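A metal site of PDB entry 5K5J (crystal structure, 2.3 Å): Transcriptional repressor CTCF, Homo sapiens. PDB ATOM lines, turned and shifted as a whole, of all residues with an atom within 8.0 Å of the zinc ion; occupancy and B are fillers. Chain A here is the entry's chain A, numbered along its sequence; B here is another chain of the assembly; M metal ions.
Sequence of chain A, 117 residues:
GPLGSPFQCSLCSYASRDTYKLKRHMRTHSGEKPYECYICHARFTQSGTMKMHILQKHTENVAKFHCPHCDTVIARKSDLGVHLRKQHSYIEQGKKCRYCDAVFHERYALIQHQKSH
The backbone NH of Ala 42 lies close to the side-chain sulfur of Cys 40. SG of Cys 37 lies close to N of Ile 39, at 3.4 Å. A ring nitrogen (ND1) of His 53 sits at hydrogen-bond distance from OP1 of DA 6 of chain B, at 2.7 Å. The backbone carbonyl oxygen (O) of Ala 42 is in hydrogen-bond range of the backbone NH (N) of Cys 37 (2.8 Å).
Within 4 Å of the zinc ion: Cys 37, Cys 40, His 53 and His 58.
The zinc ion is bound by NE2 of His 58 (2.0 Å). The zinc ion is bound by a ring nitrogen (NE2) of His 53. SG of Cys 40 binds the zinc ion (2.3 Å). SG of Cys 37 is bound to the zinc ion, 2.3 Å away. The zinc ion has four donor atoms within binding distance.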
ATOM      1  N   GLU A  36     -32.473  -5.533 -21.545  1.00  0.00           N
ATOM      2  CA  GLU A  36     -32.716  -6.588 -22.521  1.00  0.00           C
ATOM      3  C   GLU A  36     -33.135  -5.983 -23.853  1.00  0.00           C
ATOM      4  O   GLU A  36     -34.024  -5.123 -23.888  1.00  0.00           O
ATOM      5  CB  GLU A  36     -33.802  -7.551 -22.029  1.00  0.00           C
ATOM      6  CG  GLU A  36     -34.295  -8.524 -23.087  1.00  0.00           C
ATOM      7  CD  GLU A  36     -35.506  -9.325 -22.635  1.00  0.00           C
ATOM      8  OE1 GLU A  36     -35.629  -9.572 -21.425  1.00  0.00           O
ATOM      9  OE2 GLU A  36     -36.331  -9.688 -23.498  1.00  0.00           O
ATOM     10  N   CYS A  37     -32.486  -6.418 -24.930  1.00  0.00           N
ATOM     11  CA  CYS A  37     -32.913  -6.026 -26.264  1.00  0.00           C
ATOM     12  C   CYS A  37     -34.288  -6.625 -26.561  1.00  0.00           C
ATOM     13  O   CYS A  37     -34.492  -7.839 -26.397  1.00  0.00           O
ATOM     14  CB  CYS A  37     -31.898  -6.479 -27.309  1.00  0.00           C
ATOM     15  SG  CYS A  37     -32.376  -6.142 -29.021  1.00  0.00           S
ATOM     16  N   TYR A  38     -35.229  -5.785 -26.975  1.00  0.00           N
ATOM     17  CA  TYR A  38     -36.582  -6.281 -27.228  1.00  0.00           C
ATOM     18  C   TYR A  38     -36.687  -7.090 -28.521  1.00  0.00           C
ATOM     19  O   TYR A  38     -37.757  -7.637 -28.796  1.00  0.00           O
ATOM     20  CB  TYR A  38     -37.574  -5.120 -27.259  1.00  0.00           C
ATOM     21  CG  TYR A  38     -37.450  -4.233 -28.477  1.00  0.00           C
ATOM     22  CD1 TYR A  38     -36.478  -3.244 -28.557  1.00  0.00           C
ATOM     23  CD2 TYR A  38     -38.309  -4.392 -29.561  1.00  0.00           C
ATOM     24  CE1 TYR A  38     -36.363  -2.438 -29.671  1.00  0.00           C
ATOM     25  CE2 TYR A  38     -38.207  -3.586 -30.682  1.00  0.00           C
ATOM     26  CZ  TYR A  38     -37.236  -2.615 -30.733  1.00  0.00           C
ATOM     27  OH  TYR A  38     -37.126  -1.803 -31.840  1.00  0.00           O
ATOM     28  N   ILE A  39     -35.616  -7.193 -29.298  1.00  0.00           N
ATOM     29  CA  ILE A  39     -35.660  -7.881 -30.580  1.00  0.00           C
ATOM     30  C   ILE A  39     -35.028  -9.267 -30.462  1.00  0.00           C
ATOM     31  O   ILE A  39     -35.709 -10.282 -30.652  1.00  0.00           O
ATOM     32  CB  ILE A  39     -34.958  -7.057 -31.680  1.00  0.00           C
ATOM     33  CG1 ILE A  39     -35.626  -5.688 -31.807  1.00  0.00           C
ATOM     34  CG2 ILE A  39     -34.984  -7.803 -33.004  1.00  0.00           C
ATOM     35  CD1 ILE A  39     -34.977  -4.779 -32.823  1.00  0.00           C
ATOM     36  N   CYS A  40     -33.740  -9.327 -30.139  1.00  0.00           N
ATOM     37  CA  CYS A  40     -33.025 -10.586 -30.030  1.00  0.00           C
ATOM     38  C   CYS A  40     -32.930 -11.088 -28.599  1.00  0.00           C
ATOM     39  O   CYS A  40     -32.413 -12.198 -28.378  1.00  0.00           O
ATOM     40  CB  CYS A  40     -31.616 -10.453 -30.613  1.00  0.00           C
ATOM     41  SG  CYS A  40     -30.487  -9.456 -29.616  1.00  0.00           S
ATOM     42  N   HIS A  41     -33.399 -10.311 -27.617  1.00  0.00           N
ATOM     43  CA  HIS A  41     -33.470 -10.698 -26.215  1.00  0.00           C
ATOM     44  C   HIS A  41     -32.085 -10.933 -25.598  1.00  0.00           C
ATOM     45  O   HIS A  41     -31.969 -11.657 -24.608  1.00  0.00           O
ATOM     46  CB  HIS A  41     -34.358 -11.936 -26.020  1.00  0.00           C
ATOM     47  CG  HIS A  41     -35.787 -11.691 -26.398  1.00  0.00           C
ATOM     48  ND1 HIS A  41     -36.668 -11.029 -25.571  1.00  0.00           N
ATOM     49  CD2 HIS A  41     -36.490 -12.017 -27.504  1.00  0.00           C
ATOM     50  CE1 HIS A  41     -37.854 -10.955 -26.159  1.00  0.00           C
ATOM     51  NE2 HIS A  41     -37.765 -11.546 -27.334  1.00  0.00           N
ATOM     52  N   ALA A  42     -31.041 -10.322 -26.159  1.00  0.00           N
ATOM     53  CA  ALA A  42     -29.761 -10.292 -25.496  1.00  0.00           C
ATOM     54  C   ALA A  42     -29.797  -9.308 -24.321  1.00  0.00           C
ATOM     55  O   ALA A  42     -30.637  -8.402 -24.276  1.00  0.00           O
ATOM     56  CB  ALA A  42     -28.647  -9.902 -26.466  1.00  0.00           C
ATOM     57  N   ARG A  43     -28.894  -9.494 -23.373  1.00  0.00           N
ATOM     58  CA  ARG A  43     -28.888  -8.713 -22.149  1.00  0.00           C
ATOM     59  C   ARG A  43     -27.559  -7.986 -21.987  1.00  0.00           C
ATOM     60  O   ARG A  43     -26.525  -8.420 -22.500  1.00  0.00           O
ATOM     61  CB  ARG A  43     -29.154  -9.607 -20.930  1.00  0.00           C
ATOM     62  CG  ARG A  43     -30.398 -10.472 -21.082  1.00  0.00           C
ATOM     63  CD  ARG A  43     -30.808 -11.101 -19.769  1.00  0.00           C
ATOM     64  NE  ARG A  43     -31.215 -10.099 -18.789  1.00  0.00           N
ATOM     65  CZ  ARG A  43     -32.442  -9.604 -18.695  1.00  0.00           C
ATOM     66  NH1 ARG A  43     -33.391 -10.019 -19.523  1.00  0.00           N
ATOM     67  NH2 ARG A  43     -32.719  -8.693 -17.774  1.00  0.00           N
ATOM     68  N   PHE A  44     -27.614  -6.855 -21.280  1.00  0.00           N
ATOM     69  CA  PHE A  44     -26.471  -5.948 -21.168  1.00  0.00           C
ATOM     70  C   PHE A  44     -26.427  -5.336 -19.780  1.00  0.00           C
ATOM     71  O   PHE A  44     -27.434  -5.267 -19.064  1.00  0.00           O
ATOM     72  CB  PHE A  44     -26.530  -4.848 -22.231  1.00  0.00           C
ATOM     73  CG  PHE A  44     -26.819  -5.357 -23.615  1.00  0.00           C
ATOM     74  CD1 PHE A  44     -25.811  -5.800 -24.441  1.00  0.00           C
ATOM     75  CD2 PHE A  44     -28.130  -5.412 -24.075  1.00  0.00           C
ATOM     76  CE1 PHE A  44     -26.077  -6.281 -25.704  1.00  0.00           C
ATOM     77  CE2 PHE A  44     -28.412  -5.887 -25.338  1.00  0.00           C
ATOM     78  CZ  PHE A  44     -27.384  -6.324 -26.156  1.00  0.00           C
ATOM     79  N   MET A  50     -26.960  -1.296 -24.545  1.00  0.00           N
ATOM     80  CA  MET A  50     -28.072  -1.868 -25.289  1.00  0.00           C
ATOM     81  C   MET A  50     -28.444  -0.993 -26.482  1.00  0.00           C
ATOM     82  O   MET A  50     -28.743  -1.510 -27.577  1.00  0.00           O
ATOM     83  CB  MET A  50     -29.273  -2.061 -24.365  1.00  0.00           C
ATOM     84  CG  MET A  50     -30.531  -2.536 -25.066  1.00  0.00           C
ATOM     85  SD  MET A  50     -31.919  -2.725 -23.916  1.00  0.00           S
ATOM     86  CE  MET A  50     -32.134  -1.044 -23.347  1.00  0.00           C
ATOM     87  N   HIS A  53     -26.057  -1.558 -29.204  1.00  0.00           N
ATOM     88  CA  HIS A  53     -26.324  -2.870 -29.780  1.00  0.00           C
ATOM     89  C   HIS A  53     -27.465  -2.811 -30.790  1.00  0.00           C
ATOM     90  O   HIS A  53     -27.363  -3.356 -31.894  1.00  0.00           O
ATOM     91  CB  HIS A  53     -26.642  -3.872 -28.678  1.00  0.00           C
ATOM     92  CG  HIS A  53     -27.338  -5.104 -29.160  1.00  0.00           C
ATOM     93  ND1 HIS A  53     -26.667  -6.185 -29.689  1.00  0.00           N
ATOM     94  CD2 HIS A  53     -28.657  -5.422 -29.191  1.00  0.00           C
ATOM     95  CE1 HIS A  53     -27.541  -7.124 -30.022  1.00  0.00           C
ATOM     96  NE2 HIS A  53     -28.757  -6.677 -29.737  1.00  0.00           N
ATOM     97  N   ILE A  54     -28.561  -2.139 -30.426  1.00  0.00           N
ATOM     98  CA  ILE A  54     -29.707  -2.045 -31.337  1.00  0.00           C
ATOM     99  C   ILE A  54     -29.354  -1.204 -32.559  1.00  0.00           C
ATOM    100  O   ILE A  54     -29.845  -1.484 -33.668  1.00  0.00           O
ATOM    101  CB  ILE A  54     -30.925  -1.475 -30.577  1.00  0.00           C
ATOM    102  CG1 ILE A  54     -31.284  -2.374 -29.398  1.00  0.00           C
ATOM    103  CG2 ILE A  54     -32.114  -1.318 -31.511  1.00  0.00           C
ATOM    104  CD1 ILE A  54     -32.502  -1.925 -28.624  1.00  0.00           C
ATOM    105  N   LEU A  55     -28.496  -0.194 -32.397  1.00  0.00           N
ATOM    106  CA  LEU A  55     -28.097   0.612 -33.546  1.00  0.00           C
ATOM    107  C   LEU A  55     -27.213  -0.182 -34.508  1.00  0.00           C
ATOM    108  O   LEU A  55     -27.388  -0.103 -35.727  1.00  0.00           O
ATOM    109  CB  LEU A  55     -27.368   1.867 -33.076  1.00  0.00           C
ATOM    110  CG  LEU A  55     -26.862   2.812 -34.170  1.00  0.00           C
ATOM    111  CD1 LEU A  55     -28.027   3.504 -34.864  1.00  0.00           C
ATOM    112  CD2 LEU A  55     -25.867   3.824 -33.618  1.00  0.00           C
ATOM    113  N   LYS A  57     -26.774  -3.592 -34.706  1.00  0.00           N
ATOM    114  CA  LYS A  57     -27.216  -4.929 -35.099  1.00  0.00           C
ATOM    115  C   LYS A  57     -28.619  -4.965 -35.691  1.00  0.00           C
ATOM    116  O   LYS A  57     -28.875  -5.802 -36.553  1.00  0.00           O
ATOM    117  CB  LYS A  57     -27.164  -5.874 -33.894  1.00  0.00           C
ATOM    118  CG  LYS A  57     -25.798  -5.965 -33.235  1.00  0.00           C
ATOM    119  CD  LYS A  57     -24.840  -6.842 -34.024  1.00  0.00           C
ATOM    120  CE  LYS A  57     -24.852  -8.266 -33.505  1.00  0.00           C
ATOM    121  NZ  LYS A  57     -24.472  -8.324 -32.057  1.00  0.00           N
ATOM    122  N   HIS A  58     -29.519  -4.092 -35.253  1.00  0.00           N
ATOM    123  CA  HIS A  58     -30.912  -4.153 -35.674  1.00  0.00           C
ATOM    124  C   HIS A  58     -31.400  -2.923 -36.424  1.00  0.00           C
ATOM    125  O   HIS A  58     -32.590  -2.846 -36.756  1.00  0.00           O
ATOM    126  CB  HIS A  58     -31.821  -4.383 -34.459  1.00  0.00           C
ATOM    127  CG  HIS A  58     -31.439  -5.573 -33.637  1.00  0.00           C
ATOM    128  ND1 HIS A  58     -31.593  -6.863 -34.086  1.00  0.00           N
ATOM    129  CD2 HIS A  58     -30.923  -5.669 -32.388  1.00  0.00           C
ATOM    130  CE1 HIS A  58     -31.180  -7.707 -33.153  1.00  0.00           C
ATOM    131  NE2 HIS A  58     -30.760  -7.011 -32.115  1.00  0.00           N
ATOM    132  P    DA B   6     -23.039  -6.404 -28.808  1.00  0.00           P
ATOM    133  OP1  DA B   6     -24.217  -7.245 -29.113  1.00  0.00           O
ATOM    134  OP2  DA B   6     -23.060  -4.963 -29.145  1.00  0.00           O
ATOM    135  O5'  DA B   6     -22.708  -6.572 -27.258  1.00  0.00           O
ATOM    136  C5'  DA B   6     -22.369  -7.852 -26.749  1.00  0.00           C
ATOM    137  C4'  DA B   6     -21.560  -7.723 -25.470  1.00  0.00           C
ATOM    138  O4'  DA B   6     -20.354  -6.947 -25.732  1.00  0.00           O
ATOM    139  C3'  DA B   6     -22.278  -7.040 -24.310  1.00  0.00           C
ATOM    140  O3'  DA B   6     -22.049  -7.783 -23.116  1.00  0.00           O
ATOM    141  C2'  DA B   6     -21.650  -5.643 -24.269  1.00  0.00           C
ATOM    142  C1'  DA B   6     -20.251  -5.880 -24.812  1.00  0.00           C
ATOM    143  N9   DA B   6     -19.714  -4.731 -25.534  1.00  0.00           N
ATOM    144  C8   DA B   6     -20.374  -3.939 -26.423  1.00  0.00           C
ATOM    145  N7   DA B   6     -19.635  -2.970 -26.925  1.00  0.00           N
ATOM    146  C5   DA B   6     -18.401  -3.147 -26.322  1.00  0.00           C
ATOM    147  C6   DA B   6     -17.183  -2.453 -26.421  1.00  0.00           C
ATOM    148  N6   DA B   6     -17.010  -1.390 -27.218  1.00  0.00           N
ATOM    149  N1   DA B   6     -16.151  -2.891 -25.688  1.00  0.00           N
ATOM    150  C2   DA B   6     -16.320  -3.960 -24.898  1.00  0.00           C
ATOM    151  N3   DA B   6     -17.420  -4.690 -24.709  1.00  0.00           N
ATOM    152  C4   DA B   6     -18.438  -4.234 -25.462  1.00  0.00           C
HETATM  153 ZN    ZN M   1     -30.684  -7.252 -30.117  1.00  0.00          ZN
